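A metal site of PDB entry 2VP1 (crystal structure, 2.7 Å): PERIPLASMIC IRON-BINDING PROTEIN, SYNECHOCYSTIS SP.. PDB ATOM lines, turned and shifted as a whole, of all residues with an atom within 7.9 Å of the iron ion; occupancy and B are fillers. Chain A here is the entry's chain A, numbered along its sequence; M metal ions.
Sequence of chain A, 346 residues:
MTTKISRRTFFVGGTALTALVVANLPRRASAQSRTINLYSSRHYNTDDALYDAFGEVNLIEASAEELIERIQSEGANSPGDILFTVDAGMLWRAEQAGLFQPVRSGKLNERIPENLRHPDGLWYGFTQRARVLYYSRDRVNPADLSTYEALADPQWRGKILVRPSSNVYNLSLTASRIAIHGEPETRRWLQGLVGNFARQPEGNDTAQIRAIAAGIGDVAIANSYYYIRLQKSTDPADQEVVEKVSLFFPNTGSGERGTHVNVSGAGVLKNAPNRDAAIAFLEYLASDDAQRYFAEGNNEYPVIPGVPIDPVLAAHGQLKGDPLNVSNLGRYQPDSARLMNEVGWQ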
ATOM      1  N   SER A  41      16.971  21.955  -5.960  1.00  0.00           N
ATOM      2  CA  SER A  41      15.778  22.414  -6.669  1.00  0.00           C
ATOM      3  C   SER A  41      15.692  21.808  -8.079  1.00  0.00           C
ATOM      4  O   SER A  41      14.759  22.122  -8.818  1.00  0.00           O
ATOM      5  CB  SER A  41      15.688  23.940  -6.703  1.00  0.00           C
ATOM      6  OG  SER A  41      16.362  24.487  -7.833  1.00  0.00           O
ATOM      7  N   ARG A  42      16.667  20.973  -8.454  1.00  0.00           N
ATOM      8  CA  ARG A  42      16.555  20.215  -9.713  1.00  0.00           C
ATOM      9  C   ARG A  42      15.335  19.277  -9.713  1.00  0.00           C
ATOM     10  O   ARG A  42      14.854  18.877  -8.648  1.00  0.00           O
ATOM     11  CB  ARG A  42      17.848  19.439 -10.013  1.00  0.00           C
ATOM     12  CG  ARG A  42      18.961  20.300 -10.604  1.00  0.00           C
ATOM     13  CD  ARG A  42      20.174  19.484 -10.915  1.00  0.00           C
ATOM     14  NE  ARG A  42      20.001  18.685 -12.123  1.00  0.00           N
ATOM     15  CZ  ARG A  42      20.507  18.989 -13.318  1.00  0.00           C
ATOM     16  NH1 ARG A  42      21.223  20.095 -13.467  1.00  0.00           N
ATOM     17  NH2 ARG A  42      20.297  18.197 -14.363  1.00  0.00           N
ATOM     18  N   HIS A  43      14.840  18.928 -10.894  1.00  0.00           N
ATOM     19  CA  HIS A  43      13.583  18.185 -11.000  1.00  0.00           C
ATOM     20  C   HIS A  43      13.607  17.159 -12.143  1.00  0.00           C
ATOM     21  O   HIS A  43      12.688  17.093 -12.967  1.00  0.00           O
ATOM     22  CB  HIS A  43      12.410  19.157 -11.217  1.00  0.00           C
ATOM     23  CG  HIS A  43      12.727  20.277 -12.164  1.00  0.00           C
ATOM     24  ND1 HIS A  43      12.980  21.562 -11.744  1.00  0.00           N
ATOM     25  CD2 HIS A  43      12.878  20.294 -13.513  1.00  0.00           C
ATOM     26  CE1 HIS A  43      13.250  22.333 -12.783  1.00  0.00           C
ATOM     27  NE2 HIS A  43      13.192  21.592 -13.873  1.00  0.00           N
ATOM     28  N   TYR A  44      14.660  16.352 -12.193  1.00  0.00           N
ATOM     29  CA  TYR A  44      14.831  15.393 -13.257  1.00  0.00           C
ATOM     30  C   TYR A  44      15.058  14.040 -12.652  1.00  0.00           C
ATOM     31  O   TYR A  44      16.042  13.834 -11.941  1.00  0.00           O
ATOM     32  CB  TYR A  44      16.006  15.786 -14.153  1.00  0.00           C
ATOM     33  CG  TYR A  44      15.979  17.243 -14.505  1.00  0.00           C
ATOM     34  CD1 TYR A  44      15.044  17.737 -15.432  1.00  0.00           C
ATOM     35  CD2 TYR A  44      16.846  18.137 -13.895  1.00  0.00           C
ATOM     36  CE1 TYR A  44      14.996  19.104 -15.742  1.00  0.00           C
ATOM     37  CE2 TYR A  44      16.808  19.502 -14.194  1.00  0.00           C
ATOM     38  CZ  TYR A  44      15.883  19.967 -15.126  1.00  0.00           C
ATOM     39  OH  TYR A  44      15.854  21.305 -15.441  1.00  0.00           O
ATOM     40  N   VAL A  86      18.680  25.312 -10.334  1.00  0.00           N
ATOM     41  CA  VAL A  86      18.606  25.350 -11.799  1.00  0.00           C
ATOM     42  C   VAL A  86      18.574  26.792 -12.277  1.00  0.00           C
ATOM     43  O   VAL A  86      18.156  27.063 -13.392  1.00  0.00           O
ATOM     44  CB  VAL A  86      17.378  24.601 -12.385  1.00  0.00           C
ATOM     45  CG1 VAL A  86      17.553  23.116 -12.247  1.00  0.00           C
ATOM     46  CG2 VAL A  86      16.072  25.075 -11.748  1.00  0.00           C
ATOM     47  N   ARG A 129      21.709  26.226 -20.180  1.00  0.00           N
ATOM     48  CA  ARG A 129      20.422  25.910 -20.793  1.00  0.00           C
ATOM     49  C   ARG A 129      19.823  27.171 -21.359  1.00  0.00           C
ATOM     50  O   ARG A 129      19.960  28.248 -20.771  1.00  0.00           O
ATOM     51  CB  ARG A 129      19.434  25.247 -19.810  1.00  0.00           C
ATOM     52  CG  ARG A 129      19.124  26.029 -18.533  1.00  0.00           C
ATOM     53  CD  ARG A 129      19.928  25.546 -17.313  1.00  0.00           C
ATOM     54  NE  ARG A 129      19.674  24.146 -16.950  1.00  0.00           N
ATOM     55  CZ  ARG A 129      18.534  23.677 -16.434  1.00  0.00           C
ATOM     56  NH1 ARG A 129      17.485  24.475 -16.233  1.00  0.00           N
ATOM     57  NH2 ARG A 129      18.413  22.392 -16.135  1.00  0.00           N
ATOM     58  N   ARG A 131      16.553  29.326 -22.726  1.00  0.00           N
ATOM     59  CA  ARG A 131      15.101  29.575 -22.701  1.00  0.00           C
ATOM     60  C   ARG A 131      14.685  29.919 -24.128  1.00  0.00           C
ATOM     61  O   ARG A 131      14.832  31.062 -24.588  1.00  0.00           O
ATOM     62  CB  ARG A 131      14.743  30.704 -21.734  1.00  0.00           C
ATOM     63  CG  ARG A 131      13.314  30.680 -21.262  1.00  0.00           C
ATOM     64  CD  ARG A 131      13.196  30.390 -19.764  1.00  0.00           C
ATOM     65  NE  ARG A 131      11.809  30.332 -19.328  1.00  0.00           N
ATOM     66  CZ  ARG A 131      11.134  29.191 -19.205  1.00  0.00           C
ATOM     67  NH1 ARG A 131      11.744  28.034 -19.465  1.00  0.00           N
ATOM     68  NH2 ARG A 131       9.858  29.196 -18.825  1.00  0.00           N
ATOM     69  N   ARG A 163       4.497  28.932 -18.634  1.00  0.00           N
ATOM     70  CA  ARG A 163       4.165  28.537 -17.287  1.00  0.00           C
ATOM     71  C   ARG A 163       4.056  29.733 -16.286  1.00  0.00           C
ATOM     72  O   ARG A 163       4.499  30.863 -16.614  1.00  0.00           O
ATOM     73  CB  ARG A 163       5.198  27.524 -16.818  1.00  0.00           C
ATOM     74  CG  ARG A 163       6.471  28.132 -16.341  1.00  0.00           C
ATOM     75  CD  ARG A 163       7.529  27.085 -16.265  1.00  0.00           C
ATOM     76  NE  ARG A 163       7.267  26.180 -15.171  1.00  0.00           N
ATOM     77  CZ  ARG A 163       8.054  25.170 -14.833  1.00  0.00           C
ATOM     78  NH1 ARG A 163       9.152  24.922 -15.534  1.00  0.00           N
ATOM     79  NH2 ARG A 163       7.725  24.411 -13.803  1.00  0.00           N
ATOM     80  N   ASN A 167       7.627  30.729 -11.285  1.00  0.00           N
ATOM     81  CA  ASN A 167       8.736  29.913 -11.753  1.00  0.00           C
ATOM     82  C   ASN A 167      10.027  30.673 -12.031  1.00  0.00           C
ATOM     83  O   ASN A 167      10.069  31.785 -12.592  1.00  0.00           O
ATOM     84  CB  ASN A 167       8.413  29.074 -12.975  1.00  0.00           C
ATOM     85  CG  ASN A 167       9.526  28.096 -13.291  1.00  0.00           C
ATOM     86  OD1 ASN A 167      10.359  28.354 -14.137  1.00  0.00           O
ATOM     87  ND2 ASN A 167       9.578  27.009 -12.548  1.00  0.00           N
ATOM     88  N   VAL A 168      11.094  30.004 -11.655  1.00  0.00           N
ATOM     89  CA  VAL A 168      12.401  30.589 -11.569  1.00  0.00           C
ATOM     90  C   VAL A 168      12.935  30.921 -12.952  1.00  0.00           C
ATOM     91  O   VAL A 168      13.652  31.923 -13.142  1.00  0.00           O
ATOM     92  CB  VAL A 168      13.320  29.661 -10.719  1.00  0.00           C
ATOM     93  CG1 VAL A 168      13.882  28.483 -11.536  1.00  0.00           C
ATOM     94  CG2 VAL A 168      14.374  30.471 -10.037  1.00  0.00           C
ATOM     95  N   TYR A 169      12.542  30.115 -13.934  1.00  0.00           N
ATOM     96  CA  TYR A 169      12.966  30.325 -15.325  1.00  0.00           C
ATOM     97  C   TYR A 169      12.436  31.634 -15.869  1.00  0.00           C
ATOM     98  O   TYR A 169      13.162  32.375 -16.540  1.00  0.00           O
ATOM     99  CB  TYR A 169      12.531  29.157 -16.230  1.00  0.00           C
ATOM    100  CG  TYR A 169      13.086  27.808 -15.836  1.00  0.00           C
ATOM    101  CD1 TYR A 169      14.334  27.674 -15.223  1.00  0.00           C
ATOM    102  CD2 TYR A 169      12.376  26.641 -16.097  1.00  0.00           C
ATOM    103  CE1 TYR A 169      14.840  26.431 -14.850  1.00  0.00           C
ATOM    104  CE2 TYR A 169      12.872  25.387 -15.727  1.00  0.00           C
ATOM    105  CZ  TYR A 169      14.110  25.295 -15.116  1.00  0.00           C
ATOM    106  OH  TYR A 169      14.588  24.050 -14.786  1.00  0.00           O
ATOM    107  N   ASN A 204       4.221  22.793 -16.354  1.00  0.00           N
ATOM    108  CA  ASN A 204       5.648  23.103 -16.523  1.00  0.00           C
ATOM    109  C   ASN A 204       6.013  23.496 -17.961  1.00  0.00           C
ATOM    110  O   ASN A 204       5.135  23.737 -18.794  1.00  0.00           O
ATOM    111  CB  ASN A 204       6.511  21.927 -16.063  1.00  0.00           C
ATOM    112  CG  ASN A 204       5.990  20.581 -16.546  1.00  0.00           C
ATOM    113  OD1 ASN A 204       5.441  20.460 -17.643  1.00  0.00           O
ATOM    114  ND2 ASN A 204       6.138  19.559 -15.715  1.00  0.00           N
ATOM    115  N   ASP A 205       7.306  23.575 -18.253  1.00  0.00           N
ATOM    116  CA  ASP A 205       7.757  23.899 -19.600  1.00  0.00           C
ATOM    117  C   ASP A 205       7.205  22.869 -20.593  1.00  0.00           C
ATOM    118  O   ASP A 205       6.613  23.258 -21.589  1.00  0.00           O
ATOM    119  CB  ASP A 205       9.271  23.956 -19.673  1.00  0.00           C
ATOM    120  CG  ASP A 205       9.847  25.323 -19.295  1.00  0.00           C
ATOM    121  OD1 ASP A 205       9.082  26.241 -18.916  1.00  0.00           O
ATOM    122  OD2 ASP A 205      11.091  25.472 -19.381  1.00  0.00           O
ATOM    123  N   ASN A 223      12.450  25.872 -21.933  1.00  0.00           N
ATOM    124  CA  ASN A 223      13.883  25.548 -21.994  1.00  0.00           C
ATOM    125  C   ASN A 223      14.195  24.511 -23.068  1.00  0.00           C
ATOM    126  O   ASN A 223      13.375  23.623 -23.349  1.00  0.00           O
ATOM    127  CB  ASN A 223      14.392  25.068 -20.642  1.00  0.00           C
ATOM    128  CG  ASN A 223      14.533  26.191 -19.625  1.00  0.00           C
ATOM    129  OD1 ASN A 223      14.425  27.378 -19.953  1.00  0.00           O
ATOM    130  ND2 ASN A 223      14.775  25.808 -18.366  1.00  0.00           N
ATOM    131  N   TYR A 225      16.357  21.919 -23.331  1.00  0.00           N
ATOM    132  CA  TYR A 225      16.607  20.499 -23.055  1.00  0.00           C
ATOM    133  C   TYR A 225      15.321  19.644 -22.908  1.00  0.00           C
ATOM    134  O   TYR A 225      15.366  18.426 -23.038  1.00  0.00           O
ATOM    135  CB  TYR A 225      17.490  20.356 -21.794  1.00  0.00           C
ATOM    136  CG  TYR A 225      16.873  21.050 -20.597  1.00  0.00           C
ATOM    137  CD1 TYR A 225      15.922  20.396 -19.815  1.00  0.00           C
ATOM    138  CD2 TYR A 225      17.211  22.375 -20.277  1.00  0.00           C
ATOM    139  CE1 TYR A 225      15.331  21.035 -18.751  1.00  0.00           C
ATOM    140  CE2 TYR A 225      16.618  23.020 -19.191  1.00  0.00           C
ATOM    141  CZ  TYR A 225      15.679  22.341 -18.435  1.00  0.00           C
ATOM    142  OH  TYR A 225      15.057  22.937 -17.359  1.00  0.00           O
ATOM    143  N   TYR A 226      14.189  20.293 -22.628  1.00  0.00           N
ATOM    144  CA  TYR A 226      12.923  19.592 -22.490  1.00  0.00           C
ATOM    145  C   TYR A 226      12.494  19.028 -23.814  1.00  0.00           C
ATOM    146  O   TYR A 226      11.915  17.931 -23.862  1.00  0.00           O
ATOM    147  CB  TYR A 226      11.822  20.537 -21.955  1.00  0.00           C
ATOM    148  CG  TYR A 226      11.924  20.862 -20.467  1.00  0.00           C
ATOM    149  CD1 TYR A 226      11.837  19.862 -19.497  1.00  0.00           C
ATOM    150  CD2 TYR A 226      12.088  22.174 -20.035  1.00  0.00           C
ATOM    151  CE1 TYR A 226      11.926  20.154 -18.150  1.00  0.00           C
ATOM    152  CE2 TYR A 226      12.186  22.486 -18.682  1.00  0.00           C
ATOM    153  CZ  TYR A 226      12.100  21.469 -17.736  1.00  0.00           C
ATOM    154  OH  TYR A 226      12.178  21.761 -16.389  1.00  0.00           O
ATOM    155  N   ARG A 229      14.571  15.781 -24.987  1.00  0.00           N
ATOM    156  CA  ARG A 229      14.034  14.618 -24.292  1.00  0.00           C
ATOM    157  C   ARG A 229      12.865  13.996 -25.104  1.00  0.00           C
ATOM    158  O   ARG A 229      12.792  12.776 -25.280  1.00  0.00           O
ATOM    159  CB  ARG A 229      13.619  15.023 -22.869  1.00  0.00           C
ATOM    160  CG  ARG A 229      12.908  13.948 -22.061  1.00  0.00           C
ATOM    161  CD  ARG A 229      13.342  14.024 -20.590  1.00  0.00           C
ATOM    162  NE  ARG A 229      12.417  14.759 -19.712  1.00  0.00           N
ATOM    163  CZ  ARG A 229      12.810  15.610 -18.751  1.00  0.00           C
ATOM    164  NH1 ARG A 229      11.900  16.223 -17.979  1.00  0.00           N
ATOM    165  NH2 ARG A 229      14.104  15.867 -18.558  1.00  0.00           N
ATOM    166  N   ASN A 298      20.314  14.418 -19.733  1.00  0.00           N
ATOM    167  CA  ASN A 298      19.305  15.461 -19.532  1.00  0.00           C
ATOM    168  C   ASN A 298      19.336  16.551 -20.598  1.00  0.00           C
ATOM    169  O   ASN A 298      18.582  17.530 -20.523  1.00  0.00           O
ATOM    170  CB  ASN A 298      19.401  16.078 -18.129  1.00  0.00           C
ATOM    171  CG  ASN A 298      18.104  16.727 -17.701  1.00  0.00           C
ATOM    172  OD1 ASN A 298      17.029  16.136 -17.851  1.00  0.00           O
ATOM    173  ND2 ASN A 298      18.183  17.935 -17.160  1.00  0.00           N
ATOM    174  N   GLU A 300      21.160  18.974 -21.471  1.00  0.00           N
ATOM    175  CA  GLU A 300      21.631  20.316 -21.225  1.00  0.00           C
ATOM    176  C   GLU A 300      22.961  20.518 -21.981  1.00  0.00           C
ATOM    177  O   GLU A 300      23.474  19.579 -22.568  1.00  0.00           O
ATOM    178  CB  GLU A 300      21.763  20.547 -19.724  1.00  0.00           C
ATOM    179  CG  GLU A 300      20.425  20.464 -19.007  1.00  0.00           C
ATOM    180  CD  GLU A 300      20.557  20.318 -17.510  1.00  0.00           C
ATOM    181  OE1 GLU A 300      20.298  19.214 -16.996  1.00  0.00           O
ATOM    182  OE2 GLU A 300      20.922  21.308 -16.838  1.00  0.00           O
HETATM  183 FE    FE M   1      14.104  22.214 -15.724  1.00  0.00          FE
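The backbone NH of Tyr 169 lies within hydrogen-bond range of the side-chain amide oxygen of Asn 167 (2.8 Å). OH of Tyr 44 lies close to NH2 of Arg 129, 2.9 Å away. The guanidinium group (NH1) of Arg 129 sits close to the side-chain hydroxyl (OH) of Tyr 225 (3.1 Å). A ring nitrogen (ND1) of His 43 sits at hydrogen-bond distance from the backbone carbonyl oxygen (O) of Ser 41 (3.5 Å). The side-chain amide nitrogen of Asn 223 sits close to the side-chain hydroxyl of Tyr 225 (3.1 Å). OH of Tyr 169 sits close to NH1 of Arg 129, at 3.3 Å.
Of the 19 residues printed, 5 come within 4 Å of the iron ion. The nearest printed residue that does not touch the iron ion is Arg 129 (4.1 Å).
The iron ion is bound by OH of Tyr 44. OH of Tyr 225 is bound to the iron ion. The side-chain hydroxyl (OH) of Tyr 226 binds the iron ion, 2.1 Å away. The side-chain hydroxyl (OH) of Tyr 169 is bound to the iron ion (2.1 Å). The iron ion is bound by NE2 of His 43. The iron ion has five donor atoms within binding distance.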
